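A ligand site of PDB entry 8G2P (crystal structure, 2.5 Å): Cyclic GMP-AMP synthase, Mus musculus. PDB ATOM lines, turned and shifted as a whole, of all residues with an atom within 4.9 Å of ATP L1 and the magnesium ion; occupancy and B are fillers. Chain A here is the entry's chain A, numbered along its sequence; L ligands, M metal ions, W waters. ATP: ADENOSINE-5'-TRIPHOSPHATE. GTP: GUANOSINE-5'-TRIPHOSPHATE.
O of Ser 56 is in hydrogen-bond range of N of Lys 62, at 3.3 Å. OE1 of Glu 228 lies within salt-bridge range of NZ of Lys 281, at 2.8 Å. OE2 of Glu 228 lies within hydrogen-bond range of OH of Tyr 278. NZ of Lys 281 is in salt-bridge range of OE2 of Glu 59, 2.6 Å away.
Water W4 bridges O of Glu 68 (2.7 Å) and OG of Ser 56 (2.7 Å). Water W5 lies within hydrogen-bond range of an oxygen (O1B) of ATP L1 (2.5 Å) and the side-chain carboxylate (OE1) of Glu 59 (2.6 Å). Water W1 lies within hydrogen-bond range of O1B of ATP L1, OG of Ser 277 and N of Tyr 278. Water W2 lies within hydrogen-bond range of an oxygen (O2G) of ATP L1 (2.7 Å), the side-chain carboxylate of Glu 263 (3.0 Å) and the side-chain amino group of Lys 62 (3.0 Å). Water W6 lies within hydrogen-bond range of N of Tyr 278 (2.9 Å), O1A of ATP L1 (3.0 Å) and OG of Ser 277 (3.1 Å).
OD1 of Asp 70 lies within hydrogen-bond range of O2' of GTP L2 (2.9 Å). The side-chain hydroxyl (OG) of Ser 225 lies within hydrogen-bond range of an oxygen (O2') of ATP L1 (2.7 Å). The side-chain amino group (NZ) of Lys 259 lies within salt-bridge range of an oxygen (O2G) of ATP L1 (3.0 Å). The side-chain hydroxyl of Ser 225 lies within hydrogen-bond range of a nitrogen (N1) of GTP L2 (2.8 Å). N of Ser 56 lies close to O2B of ATP L1 (2.9 Å). NZ of Lys 281 sits at hydrogen-bond distance from O3' of ATP L1, 2.8 Å away. The side-chain hydroxyl (OG) of Ser 56 is in hydrogen-bond range of an oxygen (O2G) of ATP L1, at 2.7 Å. An oxygen (O1G) of ATP L1 sits at hydrogen-bond distance from the side-chain hydroxyl (OG) of Ser 277 (2.9 Å). The guanidinium group of Arg 221 lies within salt-bridge range of an oxygen (O1A) of GTP L2, at 2.9 Å. OE1 of Glu 228 sits at hydrogen-bond distance from O2' of ATP L1 (2.5 Å).
An oxygen (O1A) of ATP L1 is in hydrogen-bond range of an oxygen (O3') of GTP L2 (2.8 Å).
O3G of ATP L1 binds the magnesium ion, 2.0 Å away. O2B of ATP L1 is bound to the magnesium ion (2.1 Å). OD2 of Asp 70 binds the magnesium ion, 2.3 Å away. Water W4 binds the magnesium ion (2.4 Å). O2A of ATP L1 is bound to the magnesium ion, 2.4 Å away. The side-chain carboxylate (OE1) of Glu 68 is bound to the magnesium ion (2.5 Å). The magnesium ion has six donor atoms within binding distance.
Merely in contact with ATP L1: Gly 55 (3.4 Å), Tyr 278 (3.6 Å), Arg 221 (3.6 Å) and Lys 62 (3.97 Å). The nearest printed residue that does not touch ATP L1 is His 324 (4.1 Å).
Merely in contact with the magnesium ion: Ser 56. Within 4 Å of the magnesium ion: Ser 56, Glu 68 and Asp 70. The nearest printed residue that does not touch the magnesium ion is Gly 55 (4.8 Å).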
ATOM      1  N   GLY A  55     -19.867 -14.697  -1.229  1.00  0.00           N
ATOM      2  CA  GLY A  55     -19.467 -15.428  -2.420  1.00  0.00           C
ATOM      3  C   GLY A  55     -18.136 -14.934  -2.972  1.00  0.00           C
ATOM      4  O   GLY A  55     -17.444 -14.133  -2.336  1.00  0.00           O
ATOM      5  N   SER A  56     -17.818 -15.390  -4.174  1.00  0.00           N
ATOM      6  CA  SER A  56     -16.461 -15.409  -4.662  1.00  0.00           C
ATOM      7  C   SER A  56     -15.896 -14.009  -4.831  1.00  0.00           C
ATOM      8  O   SER A  56     -14.717 -13.792  -4.509  1.00  0.00           O
ATOM      9  CB  SER A  56     -16.350 -16.202  -5.939  1.00  0.00           C
ATOM     10  OG  SER A  56     -17.315 -15.768  -6.895  1.00  0.00           O
ATOM     11  N   GLU A  59     -14.868 -12.754  -1.535  1.00  0.00           N
ATOM     12  CA  GLU A  59     -13.787 -13.577  -0.982  1.00  0.00           C
ATOM     13  C   GLU A  59     -12.490 -13.461  -1.816  1.00  0.00           C
ATOM     14  O   GLU A  59     -11.467 -14.066  -1.481  1.00  0.00           O
ATOM     15  CB  GLU A  59     -14.213 -15.039  -0.940  1.00  0.00           C
ATOM     16  CG  GLU A  59     -15.431 -15.352  -0.080  1.00  0.00           C
ATOM     17  CD  GLU A  59     -16.108 -16.684  -0.429  1.00  0.00           C
ATOM     18  OE1 GLU A  59     -15.813 -17.212  -1.510  1.00  0.00           O
ATOM     19  OE2 GLU A  59     -16.919 -17.216   0.380  1.00  0.00           O
ATOM     20  N   LYS A  62     -13.073 -14.731  -7.266  1.00  0.00           N
ATOM     21  CA  LYS A  62     -13.755 -14.656  -8.534  1.00  0.00           C
ATOM     22  C   LYS A  62     -12.698 -14.719  -9.634  1.00  0.00           C
ATOM     23  O   LYS A  62     -11.700 -14.003  -9.567  1.00  0.00           O
ATOM     24  CB  LYS A  62     -14.575 -13.367  -8.636  1.00  0.00           C
ATOM     25  CG  LYS A  62     -15.365 -13.209  -9.928  1.00  0.00           C
ATOM     26  CD  LYS A  62     -16.589 -14.063  -9.957  1.00  0.00           C
ATOM     27  CE  LYS A  62     -17.302 -14.044 -11.294  1.00  0.00           C
ATOM     28  NZ  LYS A  62     -16.662 -14.923 -12.292  1.00  0.00           N
ATOM     29  N   GLU A  68     -20.280 -11.728 -11.833  1.00  0.00           N
ATOM     30  CA  GLU A  68     -21.256 -12.425 -11.019  1.00  0.00           C
ATOM     31  C   GLU A  68     -21.011 -12.052  -9.561  1.00  0.00           C
ATOM     32  O   GLU A  68     -19.937 -12.281  -9.027  1.00  0.00           O
ATOM     33  CB  GLU A  68     -21.210 -13.933 -11.320  1.00  0.00           C
ATOM     34  CG  GLU A  68     -22.498 -14.702 -11.031  1.00  0.00           C
ATOM     35  CD  GLU A  68     -22.658 -15.438  -9.702  1.00  0.00           C
ATOM     36  OE1 GLU A  68     -22.056 -15.052  -8.676  1.00  0.00           O
ATOM     37  OE2 GLU A  68     -23.395 -16.441  -9.706  1.00  0.00           O
ATOM     38  N   ASP A  70     -22.817 -11.931  -5.501  1.00  0.00           N
ATOM     39  CA  ASP A  70     -23.848 -12.504  -4.658  1.00  0.00           C
ATOM     40  C   ASP A  70     -24.057 -11.619  -3.435  1.00  0.00           C
ATOM     41  O   ASP A  70     -23.123 -11.397  -2.679  1.00  0.00           O
ATOM     42  CB  ASP A  70     -23.494 -13.943  -4.281  1.00  0.00           C
ATOM     43  CG  ASP A  70     -23.049 -14.768  -5.475  1.00  0.00           C
ATOM     44  OD1 ASP A  70     -23.880 -15.024  -6.381  1.00  0.00           O
ATOM     45  OD2 ASP A  70     -21.874 -15.144  -5.500  1.00  0.00           O
ATOM     46  N   ARG A 221     -33.259 -23.495   3.679  1.00  0.00           N
ATOM     47  CA  ARG A 221     -31.944 -24.127   3.693  1.00  0.00           C
ATOM     48  C   ARG A 221     -30.968 -23.213   4.454  1.00  0.00           C
ATOM     49  O   ARG A 221     -31.006 -21.983   4.303  1.00  0.00           O
ATOM     50  CB  ARG A 221     -31.475 -24.380   2.258  1.00  0.00           C
ATOM     51  CG  ARG A 221     -30.153 -25.153   2.142  1.00  0.00           C
ATOM     52  CD  ARG A 221     -29.602 -25.331   0.724  1.00  0.00           C
ATOM     53  NE  ARG A 221     -29.003 -24.112   0.179  1.00  0.00           N
ATOM     54  CZ  ARG A 221     -28.857 -23.844  -1.124  1.00  0.00           C
ATOM     55  NH1 ARG A 221     -29.133 -24.757  -2.037  1.00  0.00           N
ATOM     56  NH2 ARG A 221     -28.391 -22.670  -1.511  1.00  0.00           N
ATOM     57  N   LEU A 222     -30.091 -23.828   5.262  1.00  0.00           N
ATOM     58  CA  LEU A 222     -29.072 -23.091   5.995  1.00  0.00           C
ATOM     59  C   LEU A 222     -28.052 -22.496   5.035  1.00  0.00           C
ATOM     60  O   LEU A 222     -27.748 -23.100   4.010  1.00  0.00           O
ATOM     61  CB  LEU A 222     -28.361 -24.006   6.998  1.00  0.00           C
ATOM     62  CG  LEU A 222     -29.219 -24.399   8.196  1.00  0.00           C
ATOM     63  CD1 LEU A 222     -28.698 -25.636   8.890  1.00  0.00           C
ATOM     64  CD2 LEU A 222     -29.325 -23.248   9.162  1.00  0.00           C
ATOM     65  N   SER A 225     -22.528 -18.614   4.359  1.00  0.00           N
ATOM     66  CA  SER A 225     -21.759 -17.790   3.446  1.00  0.00           C
ATOM     67  C   SER A 225     -20.899 -16.789   4.195  1.00  0.00           C
ATOM     68  O   SER A 225     -19.817 -16.474   3.757  1.00  0.00           O
ATOM     69  CB  SER A 225     -22.674 -17.093   2.494  1.00  0.00           C
ATOM     70  OG  SER A 225     -23.302 -18.027   1.633  1.00  0.00           O
ATOM     71  N   GLU A 228     -17.972 -18.764   5.664  1.00  0.00           N
ATOM     72  CA  GLU A 228     -17.066 -19.118   4.585  1.00  0.00           C
ATOM     73  C   GLU A 228     -16.174 -17.921   4.191  1.00  0.00           C
ATOM     74  O   GLU A 228     -14.988 -18.065   3.932  1.00  0.00           O
ATOM     75  CB  GLU A 228     -17.887 -19.703   3.441  1.00  0.00           C
ATOM     76  CG  GLU A 228     -18.744 -20.901   3.831  1.00  0.00           C
ATOM     77  CD  GLU A 228     -19.761 -21.341   2.796  1.00  0.00           C
ATOM     78  OE1 GLU A 228     -19.722 -20.839   1.660  1.00  0.00           O
ATOM     79  OE2 GLU A 228     -20.573 -22.240   3.116  1.00  0.00           O
ATOM     80  N   LYS A 259     -11.823 -24.153  -9.540  1.00  0.00           N
ATOM     81  CA  LYS A 259     -13.053 -23.520  -9.992  1.00  0.00           C
ATOM     82  C   LYS A 259     -13.067 -23.409 -11.504  1.00  0.00           C
ATOM     83  O   LYS A 259     -14.111 -23.615 -12.134  1.00  0.00           O
ATOM     84  CB  LYS A 259     -13.196 -22.107  -9.443  1.00  0.00           C
ATOM     85  CG  LYS A 259     -13.609 -22.048  -7.979  1.00  0.00           C
ATOM     86  CD  LYS A 259     -13.297 -20.731  -7.330  1.00  0.00           C
ATOM     87  CE  LYS A 259     -14.060 -19.573  -7.965  1.00  0.00           C
ATOM     88  NZ  LYS A 259     -15.515 -19.694  -7.790  1.00  0.00           N
ATOM     89  N   GLU A 263     -15.592 -24.772 -14.261  1.00  0.00           N
ATOM     90  CA  GLU A 263     -16.277 -23.840 -15.150  1.00  0.00           C
ATOM     91  C   GLU A 263     -16.075 -24.229 -16.625  1.00  0.00           C
ATOM     92  O   GLU A 263     -17.047 -24.272 -17.395  1.00  0.00           O
ATOM     93  CB  GLU A 263     -15.833 -22.382 -14.949  1.00  0.00           C
ATOM     94  CG  GLU A 263     -16.537 -21.632 -13.835  1.00  0.00           C
ATOM     95  CD  GLU A 263     -16.201 -20.150 -13.690  1.00  0.00           C
ATOM     96  OE1 GLU A 263     -16.069 -19.477 -14.731  1.00  0.00           O
ATOM     97  OE2 GLU A 263     -16.070 -19.647 -12.523  1.00  0.00           O
ATOM     98  N   SER A 277     -19.906 -24.829  -8.336  1.00  0.00           N
ATOM     99  CA  SER A 277     -18.671 -24.401  -7.714  1.00  0.00           C
ATOM    100  C   SER A 277     -18.656 -24.687  -6.205  1.00  0.00           C
ATOM    101  O   SER A 277     -17.590 -24.853  -5.627  1.00  0.00           O
ATOM    102  CB  SER A 277     -18.423 -22.965  -8.018  1.00  0.00           C
ATOM    103  OG  SER A 277     -19.431 -22.203  -7.435  1.00  0.00           O
ATOM    104  N   TYR A 278     -19.830 -24.758  -5.569  1.00  0.00           N
ATOM    105  CA  TYR A 278     -19.882 -25.060  -4.138  1.00  0.00           C
ATOM    106  C   TYR A 278     -19.257 -26.430  -3.827  1.00  0.00           C
ATOM    107  O   TYR A 278     -18.721 -26.651  -2.736  1.00  0.00           O
ATOM    108  CB  TYR A 278     -21.306 -25.001  -3.575  1.00  0.00           C
ATOM    109  CG  TYR A 278     -21.351 -24.969  -2.060  1.00  0.00           C
ATOM    110  CD1 TYR A 278     -20.779 -23.910  -1.385  1.00  0.00           C
ATOM    111  CD2 TYR A 278     -21.934 -25.976  -1.293  1.00  0.00           C
ATOM    112  CE1 TYR A 278     -20.793 -23.823  -0.006  1.00  0.00           C
ATOM    113  CE2 TYR A 278     -21.950 -25.914   0.101  1.00  0.00           C
ATOM    114  CZ  TYR A 278     -21.361 -24.839   0.747  1.00  0.00           C
ATOM    115  OH  TYR A 278     -21.291 -24.613   2.113  1.00  0.00           O
ATOM    116  N   LYS A 281     -15.629 -25.744  -3.518  1.00  0.00           N
ATOM    117  CA  LYS A 281     -15.345 -24.971  -2.305  1.00  0.00           C
ATOM    118  C   LYS A 281     -15.363 -25.862  -1.072  1.00  0.00           C
ATOM    119  O   LYS A 281     -14.466 -25.809  -0.231  1.00  0.00           O
ATOM    120  CB  LYS A 281     -16.395 -23.890  -2.066  1.00  0.00           C
ATOM    121  CG  LYS A 281     -15.989 -22.763  -1.136  1.00  0.00           C
ATOM    122  CD  LYS A 281     -17.106 -21.707  -1.109  1.00  0.00           C
ATOM    123  CE  LYS A 281     -16.734 -20.429  -0.403  1.00  0.00           C
ATOM    124  NZ  LYS A 281     -17.909 -19.590  -0.074  1.00  0.00           N
ATOM    125  N   HIS A 324     -21.130 -31.898   3.474  1.00  0.00           N
ATOM    126  CA  HIS A 324     -21.212 -30.486   3.751  1.00  0.00           C
ATOM    127  C   HIS A 324     -20.257 -30.187   4.898  1.00  0.00           C
ATOM    128  O   HIS A 324     -20.309 -30.877   5.907  1.00  0.00           O
ATOM    129  CB  HIS A 324     -22.667 -30.144   4.125  1.00  0.00           C
ATOM    130  CG  HIS A 324     -23.015 -28.717   4.022  1.00  0.00           C
ATOM    131  ND1 HIS A 324     -22.483 -27.744   4.839  1.00  0.00           N
ATOM    132  CD2 HIS A 324     -23.857 -28.101   3.201  1.00  0.00           C
ATOM    133  CE1 HIS A 324     -22.984 -26.574   4.488  1.00  0.00           C
ATOM    134  NE2 HIS A 324     -23.830 -26.772   3.502  1.00  0.00           N
HETATM  135  PG  ATP L   1     -18.747 -18.504  -8.191  1.00  0.00           P
HETATM  136  O1G ATP L   1     -18.926 -19.804  -8.963  1.00  0.00           O
HETATM  137  O2G ATP L   1     -17.566 -17.714  -8.733  1.00  0.00           O
HETATM  138  O3G ATP L   1     -20.059 -17.683  -8.231  1.00  0.00           O
HETATM  139  PB  ATP L   1     -19.392 -18.627  -5.307  1.00  0.00           P
HETATM  140  O1B ATP L   1     -18.917 -19.203  -3.991  1.00  0.00           O
HETATM  141  O2B ATP L   1     -19.822 -17.177  -5.295  1.00  0.00           O
HETATM  142  O3B ATP L   1     -18.446 -18.912  -6.581  1.00  0.00           O
HETATM  143  PA  ATP L   1     -22.215 -19.223  -6.016  1.00  0.00           P
HETATM  144  O1A ATP L   1     -22.840 -20.374  -6.745  1.00  0.00           O
HETATM  145  O2A ATP L   1     -22.223 -17.818  -6.567  1.00  0.00           O
HETATM  146  O3A ATP L   1     -20.646 -19.529  -5.802  1.00  0.00           O
HETATM  147  O5' ATP L   1     -22.823 -19.234  -4.536  1.00  0.00           O
HETATM  148  C5' ATP L   1     -22.640 -18.086  -3.661  1.00  0.00           C
HETATM  149  C4' ATP L   1     -22.501 -18.591  -2.236  1.00  0.00           C
HETATM  150  O4' ATP L   1     -23.724 -19.273  -1.824  1.00  0.00           O
HETATM  151  C3' ATP L   1     -21.365 -19.605  -1.991  1.00  0.00           C
HETATM  152  O3' ATP L   1     -20.152 -18.913  -1.674  1.00  0.00           O
HETATM  153  C2' ATP L   1     -21.879 -20.367  -0.765  1.00  0.00           C
HETATM  154  O2' ATP L   1     -21.523 -19.626   0.374  1.00  0.00           O
HETATM  155  C1' ATP L   1     -23.404 -20.366  -0.990  1.00  0.00           C
HETATM  156  N9  ATP L   1     -23.912 -21.576  -1.629  1.00  0.00           N
HETATM  157  C8  ATP L   1     -23.983 -21.838  -3.001  1.00  0.00           C
HETATM  158  N7  ATP L   1     -24.504 -23.023  -3.236  1.00  0.00           N
HETATM  159  C5  ATP L   1     -24.782 -23.551  -1.979  1.00  0.00           C
HETATM  160  C6  ATP L   1     -25.306 -24.798  -1.560  1.00  0.00           C
HETATM  161  N6  ATP L   1     -25.678 -25.747  -2.408  1.00  0.00           N
HETATM  162  N1  ATP L   1     -25.444 -25.013  -0.226  1.00  0.00           N
HETATM  163  C2  ATP L   1     -25.021 -24.065   0.627  1.00  0.00           C
HETATM  164  N3  ATP L   1     -24.509 -22.862   0.344  1.00  0.00           N
HETATM  165  C4  ATP L   1     -24.415 -22.678  -0.980  1.00  0.00           C
HETATM  166  PG  GTP L   2     -29.456 -26.331  -7.694  1.00  0.00           P
HETATM  167  O1G GTP L   2     -28.107 -25.621  -8.186  1.00  0.00           O
HETATM  168  O2G GTP L   2     -29.337 -27.125  -6.333  1.00  0.00           O
HETATM  169  O3G GTP L   2     -30.182 -27.096  -8.851  1.00  0.00           O
HETATM  170  O3B GTP L   2     -30.580 -25.221  -7.330  1.00  0.00           O
HETATM  171  PB  GTP L   2     -30.719 -23.703  -7.825  1.00  0.00           P
HETATM  172  O1B GTP L   2     -29.708 -23.505  -8.953  1.00  0.00           O
HETATM  173  O2B GTP L   2     -32.204 -23.420  -8.042  1.00  0.00           O
HETATM  174  O3A GTP L   2     -30.221 -23.021  -6.436  1.00  0.00           O
HETATM  175  PA  GTP L   2     -28.704 -22.853  -5.902  1.00  0.00           P
HETATM  176  O1A GTP L   2     -28.573 -23.669  -4.638  1.00  0.00           O
HETATM  177  O2A GTP L   2     -27.845 -23.107  -7.110  1.00  0.00           O
HETATM  178  O5' GTP L   2     -28.660 -21.266  -5.564  1.00  0.00           O
HETATM  179  C5' GTP L   2     -28.747 -20.359  -6.702  1.00  0.00           C
HETATM  180  C4' GTP L   2     -27.732 -19.249  -6.583  1.00  0.00           C
HETATM  181  O4' GTP L   2     -28.108 -18.364  -5.487  1.00  0.00           O
HETATM  182  C3' GTP L   2     -26.295 -19.661  -6.233  1.00  0.00           C
HETATM  183  O3' GTP L   2     -25.566 -19.948  -7.414  1.00  0.00           O
HETATM  184  C2' GTP L   2     -25.773 -18.371  -5.620  1.00  0.00           C
HETATM  185  O2' GTP L   2     -25.573 -17.404  -6.623  1.00  0.00           O
HETATM  186  C1' GTP L   2     -26.959 -18.012  -4.738  1.00  0.00           C
HETATM  187  N9  GTP L   2     -27.006 -18.702  -3.442  1.00  0.00           N
HETATM  188  C8  GTP L   2     -27.601 -19.899  -3.109  1.00  0.00           C
HETATM  189  N7  GTP L   2     -27.485 -20.195  -1.827  1.00  0.00           N
HETATM  190  C5  GTP L   2     -26.786 -19.128  -1.275  1.00  0.00           C
HETATM  191  C6  GTP L   2     -26.345 -18.897   0.065  1.00  0.00           C
HETATM  192  O6  GTP L   2     -26.477 -19.638   1.052  1.00  0.00           O
HETATM  193  N1  GTP L   2     -25.652 -17.674   0.177  1.00  0.00           N
HETATM  194  C2  GTP L   2     -25.365 -16.827  -0.888  1.00  0.00           C
HETATM  195  N2  GTP L   2     -24.651 -15.710  -0.635  1.00  0.00           N
HETATM  196  N3  GTP L   2     -25.793 -17.053  -2.136  1.00  0.00           N
HETATM  197  C4  GTP L   2     -26.485 -18.199  -2.264  1.00  0.00           C
HETATM  198 MG    MG M   1     -20.513 -16.195  -7.003  1.00  0.00          MG
HETATM  199  O   HOH W   1     -18.863 -21.807  -4.460  1.00  0.00           O
HETATM  200  O   HOH W   2     -15.774 -17.303 -10.737  1.00  0.00           O
HETATM  201  O   HOH W   3     -27.500 -22.236   1.132  1.00  0.00           O
HETATM  202  O   HOH W   4     -19.471 -14.087  -7.065  1.00  0.00           O
HETATM  203  O   HOH W   5     -16.453 -18.761  -3.550  1.00  0.00           O
HETATM  204  O   HOH W   6     -22.167 -23.300  -6.530  1.00  0.00           O
